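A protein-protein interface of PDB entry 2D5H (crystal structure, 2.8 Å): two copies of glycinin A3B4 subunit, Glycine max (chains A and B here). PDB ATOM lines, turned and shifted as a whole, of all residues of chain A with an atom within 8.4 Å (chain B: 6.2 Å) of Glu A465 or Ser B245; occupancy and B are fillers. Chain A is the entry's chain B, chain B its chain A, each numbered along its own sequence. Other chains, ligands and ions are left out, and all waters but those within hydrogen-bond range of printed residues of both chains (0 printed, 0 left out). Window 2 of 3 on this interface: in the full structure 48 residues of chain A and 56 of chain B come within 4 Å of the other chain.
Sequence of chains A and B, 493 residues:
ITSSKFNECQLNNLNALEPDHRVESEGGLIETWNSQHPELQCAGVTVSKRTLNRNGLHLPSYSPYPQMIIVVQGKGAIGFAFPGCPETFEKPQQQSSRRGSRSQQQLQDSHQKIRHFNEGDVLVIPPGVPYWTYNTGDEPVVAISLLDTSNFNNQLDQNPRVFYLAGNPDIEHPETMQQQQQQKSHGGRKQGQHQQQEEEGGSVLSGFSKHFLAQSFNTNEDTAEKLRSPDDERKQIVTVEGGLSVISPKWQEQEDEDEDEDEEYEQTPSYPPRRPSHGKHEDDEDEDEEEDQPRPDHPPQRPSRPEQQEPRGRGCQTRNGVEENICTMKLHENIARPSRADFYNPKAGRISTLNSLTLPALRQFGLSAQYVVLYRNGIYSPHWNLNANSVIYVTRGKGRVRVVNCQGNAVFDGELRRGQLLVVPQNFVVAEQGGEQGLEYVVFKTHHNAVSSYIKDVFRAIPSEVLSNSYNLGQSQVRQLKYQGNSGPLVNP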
ATOM      1  N   ILE A 462      21.911  17.484  -8.930  1.00  0.00           N
ATOM      2  CA  ILE A 462      21.755  17.159  -7.520  1.00  0.00           C
ATOM      3  C   ILE A 462      21.141  15.770  -7.370  1.00  0.00           C
ATOM      4  O   ILE A 462      20.145  15.449  -8.022  1.00  0.00           O
ATOM      5  CB  ILE A 462      20.854  18.190  -6.810  1.00  0.00           C
ATOM      6  CG1 ILE A 462      21.516  19.571  -6.845  1.00  0.00           C
ATOM      7  CG2 ILE A 462      20.609  17.767  -5.377  1.00  0.00           C
ATOM      8  CD1 ILE A 462      20.741  20.652  -6.112  1.00  0.00           C
ATOM      9  N   PRO A 463      21.729  14.925  -6.506  1.00  0.00           N
ATOM     10  CA  PRO A 463      21.235  13.565  -6.274  1.00  0.00           C
ATOM     11  C   PRO A 463      19.713  13.486  -6.204  1.00  0.00           C
ATOM     12  O   PRO A 463      19.049  14.415  -5.741  1.00  0.00           O
ATOM     13  CB  PRO A 463      21.902  13.184  -4.959  1.00  0.00           C
ATOM     14  CG  PRO A 463      23.232  13.847  -5.081  1.00  0.00           C
ATOM     15  CD  PRO A 463      22.860  15.223  -5.608  1.00  0.00           C
ATOM     16  N   SER A 464      19.169  12.367  -6.667  1.00  0.00           N
ATOM     17  CA  SER A 464      17.730  12.157  -6.680  1.00  0.00           C
ATOM     18  C   SER A 464      17.084  12.318  -5.306  1.00  0.00           C
ATOM     19  O   SER A 464      16.026  12.938  -5.179  1.00  0.00           O
ATOM     20  CB  SER A 464      17.425  10.767  -7.237  1.00  0.00           C
ATOM     21  OG  SER A 464      18.054  10.581  -8.494  1.00  0.00           O
ATOM     22  N   GLU A 465      17.725  11.767  -4.279  1.00  0.00           N
ATOM     23  CA  GLU A 465      17.198  11.838  -2.918  1.00  0.00           C
ATOM     24  C   GLU A 465      17.203  13.235  -2.301  1.00  0.00           C
ATOM     25  O   GLU A 465      16.390  13.531  -1.421  1.00  0.00           O
ATOM     26  CB  GLU A 465      17.977  10.894  -2.001  1.00  0.00           C
ATOM     27  CG  GLU A 465      17.906   9.436  -2.403  1.00  0.00           C
ATOM     28  CD  GLU A 465      18.451   8.518  -1.331  1.00  0.00           C
ATOM     29  OE1 GLU A 465      17.905   8.525  -0.207  1.00  0.00           O
ATOM     30  OE2 GLU A 465      19.424   7.789  -1.610  1.00  0.00           O
ATOM     31  N   VAL A 466      18.115  14.088  -2.760  1.00  0.00           N
ATOM     32  CA  VAL A 466      18.229  15.444  -2.231  1.00  0.00           C
ATOM     33  C   VAL A 466      17.005  16.311  -2.498  1.00  0.00           C
ATOM     34  O   VAL A 466      16.275  16.665  -1.569  1.00  0.00           O
ATOM     35  CB  VAL A 466      19.465  16.159  -2.803  1.00  0.00           C
ATOM     36  CG1 VAL A 466      19.573  17.557  -2.212  1.00  0.00           C
ATOM     37  CG2 VAL A 466      20.718  15.351  -2.498  1.00  0.00           C
ATOM     38  N   LEU A 467      16.788  16.656  -3.766  1.00  0.00           N
ATOM     39  CA  LEU A 467      15.649  17.487  -4.151  1.00  0.00           C
ATOM     40  C   LEU A 467      14.392  17.025  -3.422  1.00  0.00           C
ATOM     41  O   LEU A 467      13.507  17.826  -3.108  1.00  0.00           O
ATOM     42  CB  LEU A 467      15.414  17.415  -5.667  1.00  0.00           C
ATOM     43  CG  LEU A 467      16.510  17.847  -6.652  1.00  0.00           C
ATOM     44  CD1 LEU A 467      17.071  19.198  -6.237  1.00  0.00           C
ATOM     45  CD2 LEU A 467      17.617  16.807  -6.699  1.00  0.00           C
ATOM     46  N   SER A 468      14.333  15.725  -3.152  1.00  0.00           N
ATOM     47  CA  SER A 468      13.202  15.109  -2.467  1.00  0.00           C
ATOM     48  C   SER A 468      12.899  15.762  -1.123  1.00  0.00           C
ATOM     49  O   SER A 468      11.927  16.509  -0.989  1.00  0.00           O
ATOM     50  CB  SER A 468      13.481  13.622  -2.256  1.00  0.00           C
ATOM     51  OG  SER A 468      13.908  13.019  -3.463  1.00  0.00           O
ATOM     52  N   ASN A 469      13.735  15.476  -0.129  1.00  0.00           N
ATOM     53  CA  ASN A 469      13.548  16.028   1.208  1.00  0.00           C
ATOM     54  C   ASN A 469      13.643  17.544   1.196  1.00  0.00           C
ATOM     55  O   ASN A 469      13.225  18.210   2.142  1.00  0.00           O
ATOM     56  CB  ASN A 469      14.595  15.457   2.166  1.00  0.00           C
ATOM     57  CG  ASN A 469      14.572  13.942   2.216  1.00  0.00           C
ATOM     58  OD1 ASN A 469      14.829  13.272   1.214  1.00  0.00           O
ATOM     59  ND2 ASN A 469      14.261  13.392   3.388  1.00  0.00           N
ATOM     60  N   SER A 470      14.195  18.082   0.113  1.00  0.00           N
ATOM     61  CA  SER A 470      14.357  19.522  -0.042  1.00  0.00           C
ATOM     62  C   SER A 470      13.019  20.251  -0.159  1.00  0.00           C
ATOM     63  O   SER A 470      12.707  21.123   0.656  1.00  0.00           O
ATOM     64  CB  SER A 470      15.204  19.820  -1.279  1.00  0.00           C
ATOM     65  OG  SER A 470      16.437  19.124  -1.234  1.00  0.00           O
ATOM     66  N   TYR A 471      12.231  19.889  -1.170  1.00  0.00           N
ATOM     67  CA  TYR A 471      10.937  20.531  -1.397  1.00  0.00           C
ATOM     68  C   TYR A 471       9.735  19.674  -1.009  1.00  0.00           C
ATOM     69  O   TYR A 471       8.601  20.160  -1.008  1.00  0.00           O
ATOM     70  CB  TYR A 471      10.794  20.933  -2.867  1.00  0.00           C
ATOM     71  CG  TYR A 471      11.985  21.671  -3.434  1.00  0.00           C
ATOM     72  CD1 TYR A 471      13.161  20.992  -3.758  1.00  0.00           C
ATOM     73  CD2 TYR A 471      11.935  23.045  -3.658  1.00  0.00           C
ATOM     74  CE1 TYR A 471      14.257  21.664  -4.295  1.00  0.00           C
ATOM     75  CE2 TYR A 471      13.024  23.726  -4.194  1.00  0.00           C
ATOM     76  CZ  TYR A 471      14.182  23.029  -4.511  1.00  0.00           C
ATOM     77  OH  TYR A 471      15.262  23.696  -5.045  1.00  0.00           O
ATOM     78  N   ASN A 472       9.986  18.405  -0.690  1.00  0.00           N
ATOM     79  CA  ASN A 472       8.937  17.456  -0.302  1.00  0.00           C
ATOM     80  C   ASN A 472       8.244  16.854  -1.524  1.00  0.00           C
ATOM     81  O   ASN A 472       7.028  16.974  -1.680  1.00  0.00           O
ATOM     82  CB  ASN A 472       7.883  18.127   0.590  1.00  0.00           C
ATOM     83  CG  ASN A 472       8.463  18.672   1.881  1.00  0.00           C
ATOM     84  OD1 ASN A 472       7.738  19.202   2.721  1.00  0.00           O
ATOM     85  ND2 ASN A 472       9.774  18.544   2.046  1.00  0.00           N
ATOM     86  N   LEU A 473       9.021  16.205  -2.383  1.00  0.00           N
ATOM     87  CA  LEU A 473       8.477  15.580  -3.582  1.00  0.00           C
ATOM     88  C   LEU A 473       8.663  14.067  -3.508  1.00  0.00           C
ATOM     89  O   LEU A 473       9.292  13.555  -2.580  1.00  0.00           O
ATOM     90  CB  LEU A 473       9.184  16.116  -4.834  1.00  0.00           C
ATOM     91  CG  LEU A 473       9.120  17.613  -5.155  1.00  0.00           C
ATOM     92  CD1 LEU A 473       9.962  17.897  -6.393  1.00  0.00           C
ATOM     93  CD2 LEU A 473       7.679  18.042  -5.381  1.00  0.00           C
ATOM     94  N   GLN A 475       9.405  10.232  -5.847  1.00  0.00           N
ATOM     95  CA  GLN A 475      10.176   9.747  -6.989  1.00  0.00           C
ATOM     96  C   GLN A 475       9.550  10.164  -8.319  1.00  0.00           C
ATOM     97  O   GLN A 475      10.227  10.209  -9.347  1.00  0.00           O
ATOM     98  CB  GLN A 475      10.307   8.222  -6.939  1.00  0.00           C
ATOM     99  CG  GLN A 475      11.034   7.625  -8.141  1.00  0.00           C
ATOM    100  CD  GLN A 475      12.412   8.230  -8.351  1.00  0.00           C
ATOM    101  OE1 GLN A 475      13.307   8.072  -7.517  1.00  0.00           O
ATOM    102  NE2 GLN A 475      12.588   8.933  -9.465  1.00  0.00           N
ATOM    103  N   VAL A 478      10.067  14.189  -8.392  1.00  0.00           N
ATOM    104  CA  VAL A 478      11.509  14.389  -8.417  1.00  0.00           C
ATOM    105  C   VAL A 478      12.024  14.023  -9.801  1.00  0.00           C
ATOM    106  O   VAL A 478      12.616  14.853 -10.491  1.00  0.00           O
ATOM    107  CB  VAL A 478      12.216  13.516  -7.359  1.00  0.00           C
ATOM    108  CG1 VAL A 478      13.726  13.572  -7.556  1.00  0.00           C
ATOM    109  CG2 VAL A 478      11.846  14.002  -5.960  1.00  0.00           C
ATOM    110  N   LYS A 482      14.016  16.323 -12.822  1.00  0.00           N
ATOM    111  CA  LYS A 482      15.306  15.797 -13.252  1.00  0.00           C
ATOM    112  C   LYS A 482      15.253  15.233 -14.672  1.00  0.00           C
ATOM    113  O   LYS A 482      16.253  15.247 -15.392  1.00  0.00           O
ATOM    114  CB  LYS A 482      15.778  14.711 -12.277  1.00  0.00           C
ATOM    115  CG  LYS A 482      15.890  15.186 -10.831  1.00  0.00           C
ATOM    116  CD  LYS A 482      16.242  14.057  -9.854  1.00  0.00           C
ATOM    117  CE  LYS A 482      17.693  13.606  -9.974  1.00  0.00           C
ATOM    118  NZ  LYS A 482      17.967  12.873 -11.236  1.00  0.00           N
ATOM    119  N   LEU B  57      20.537  17.600   7.034  1.00  0.00           N
ATOM    120  CA  LEU B  57      20.884  18.072   5.701  1.00  0.00           C
ATOM    121  C   LEU B  57      20.770  19.586   5.634  1.00  0.00           C
ATOM    122  O   LEU B  57      19.836  20.174   6.181  1.00  0.00           O
ATOM    123  CB  LEU B  57      19.958  17.440   4.657  1.00  0.00           C
ATOM    124  CG  LEU B  57      20.110  17.903   3.204  1.00  0.00           C
ATOM    125  CD1 LEU B  57      21.538  17.691   2.726  1.00  0.00           C
ATOM    126  CD2 LEU B  57      19.136  17.131   2.328  1.00  0.00           C
ATOM    127  N   ASP B 109      21.843   6.560 -10.198  1.00  0.00           N
ATOM    128  CA  ASP B 109      21.329   7.926 -10.216  1.00  0.00           C
ATOM    129  C   ASP B 109      22.084   8.776 -11.234  1.00  0.00           C
ATOM    130  O   ASP B 109      22.776   8.248 -12.107  1.00  0.00           O
ATOM    131  CB  ASP B 109      21.459   8.560  -8.827  1.00  0.00           C
ATOM    132  CG  ASP B 109      20.570   7.897  -7.794  1.00  0.00           C
ATOM    133  OD1 ASP B 109      19.332   8.006  -7.918  1.00  0.00           O
ATOM    134  OD2 ASP B 109      21.106   7.265  -6.859  1.00  0.00           O
ATOM    135  N   GLY B 242      16.178   8.653   8.266  1.00  0.00           N
ATOM    136  CA  GLY B 242      16.329   7.498   7.403  1.00  0.00           C
ATOM    137  C   GLY B 242      17.633   7.613   6.643  1.00  0.00           C
ATOM    138  O   GLY B 242      18.331   6.624   6.426  1.00  0.00           O
ATOM    139  N   GLY B 243      17.960   8.836   6.238  1.00  0.00           N
ATOM    140  CA  GLY B 243      19.195   9.069   5.513  1.00  0.00           C
ATOM    141  C   GLY B 243      19.071   8.940   4.008  1.00  0.00           C
ATOM    142  O   GLY B 243      18.025   8.553   3.488  1.00  0.00           O
ATOM    143  N   LEU B 244      20.150   9.274   3.307  1.00  0.00           N
ATOM    144  CA  LEU B 244      20.180   9.193   1.854  1.00  0.00           C
ATOM    145  C   LEU B 244      20.914   7.933   1.420  1.00  0.00           C
ATOM    146  O   LEU B 244      22.104   7.765   1.702  1.00  0.00           O
ATOM    147  CB  LEU B 244      20.873  10.423   1.262  1.00  0.00           C
ATOM    148  CG  LEU B 244      20.134  11.762   1.336  1.00  0.00           C
ATOM    149  CD1 LEU B 244      19.902  12.162   2.784  1.00  0.00           C
ATOM    150  CD2 LEU B 244      20.952  12.820   0.617  1.00  0.00           C
ATOM    151  N   SER B 245      20.198   7.049   0.734  1.00  0.00           N
ATOM    152  CA  SER B 245      20.771   5.800   0.256  1.00  0.00           C
ATOM    153  C   SER B 245      21.988   6.065  -0.620  1.00  0.00           C
ATOM    154  O   SER B 245      22.962   5.313  -0.584  1.00  0.00           O
ATOM    155  CB  SER B 245      19.727   5.010  -0.538  1.00  0.00           C
ATOM    156  OG  SER B 245      18.582   4.742   0.253  1.00  0.00           O
ATOM    157  N   VAL B 246      21.927   7.141  -1.403  1.00  0.00           N
ATOM    158  CA  VAL B 246      23.022   7.508  -2.294  1.00  0.00           C
ATOM    159  C   VAL B 246      24.349   7.363  -1.556  1.00  0.00           C
ATOM    160  O   VAL B 246      25.279   6.720  -2.044  1.00  0.00           O
ATOM    161  CB  VAL B 246      22.883   8.964  -2.791  1.00  0.00           C
ATOM    162  CG1 VAL B 246      23.971   9.269  -3.807  1.00  0.00           C
ATOM    163  CG2 VAL B 246      21.504   9.179  -3.403  1.00  0.00           C
ATOM    164  N   ILE B 247      24.423   7.968  -0.374  1.00  0.00           N
ATOM    165  CA  ILE B 247      25.623   7.896   0.450  1.00  0.00           C
ATOM    166  C   ILE B 247      25.538   6.618   1.281  1.00  0.00           C
ATOM    167  O   ILE B 247      26.406   5.745   1.196  1.00  0.00           O
ATOM    168  CB  ILE B 247      25.733   9.119   1.399  1.00  0.00           C
ATOM    169  CG1 ILE B 247      26.021  10.393   0.594  1.00  0.00           C
ATOM    170  CG2 ILE B 247      26.834   8.892   2.421  1.00  0.00           C
ATOM    171  CD1 ILE B 247      24.882  10.844  -0.306  1.00  0.00           C
ATOM    172  N   SER B 248      24.477   6.513   2.075  1.00  0.00           N
ATOM    173  CA  SER B 248      24.259   5.346   2.920  1.00  0.00           C
ATOM    174  C   SER B 248      23.849   4.151   2.069  1.00  0.00           C
ATOM    175  O   SER B 248      24.421   3.909   1.006  1.00  0.00           O
ATOM    176  CB  SER B 248      23.169   5.639   3.954  1.00  0.00           C
ATOM    177  OG  SER B 248      22.931   4.508   4.777  1.00  0.00           O
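OD1 of Asp B109 lies within hydrogen-bond range of OG of Ser A464 (2.9 Å). The backbone NH (N) of Ser B245 is in hydrogen-bond range of the side-chain carboxylate (OE2) of Glu A465 (2.6 Å). The side-chain carboxylate of Glu A465 sits at hydrogen-bond distance from the backbone NH of Val B246 (2.6 Å).
OG of Ser A468 sits at hydrogen-bond distance from O of Ser A464 (2.7 Å). The side-chain hydroxyl (OG) of Ser A468 lies close to the backbone carbonyl oxygen (O) of Glu A465 (3.3 Å). OD1 of Asn A469 lies close to O of Glu A465.
Among the printed residues, merely in contact across the chains: Glu A465 with Leu B244 (3.1 Å) and Glu A465 with Gly B243 (3.7 Å).
Of chain A, only Glu A465 (2.6 Å) comes within 4 Å of Ser B245. Of the printed residues of chain A, Val B246 touches Glu A465 (2.6 Å). Of the printed residues of chain B, Ser A464 touches Asp B109 (2.9 Å). Tyr A471 touches none of the printed residues of chain B. Asn A469 touches none of the printed residues of chain B. The nearest residue of chain B that does not touch Glu A465 is Ile B247 (5.2 Å). The nearest residue of chain A that does not touch Ser B245 is Val A466 (8.1 Å). The nearest printed residue of chain B that does not touch Ser A464 is Val B246 (5.1 Å).
Printed residues of chain B that touch a printed residue of chain A: Asp B109, Gly B243, Leu B244, Ser B245 and Val B246. Hydrophobic or aromatic side chains of chain B within 4 Å of the printed part of chain A: Leu B244 and Val B246. Among the printed residues, no Asp or Glu carboxylate lies within 4 Å of a Lys or Arg side-chain nitrogen of the other chain.
No position is printed for both chains. Of the 5 pairs that touch across the chains among the printed residues, none has its exchanged pair printed and touching as well.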
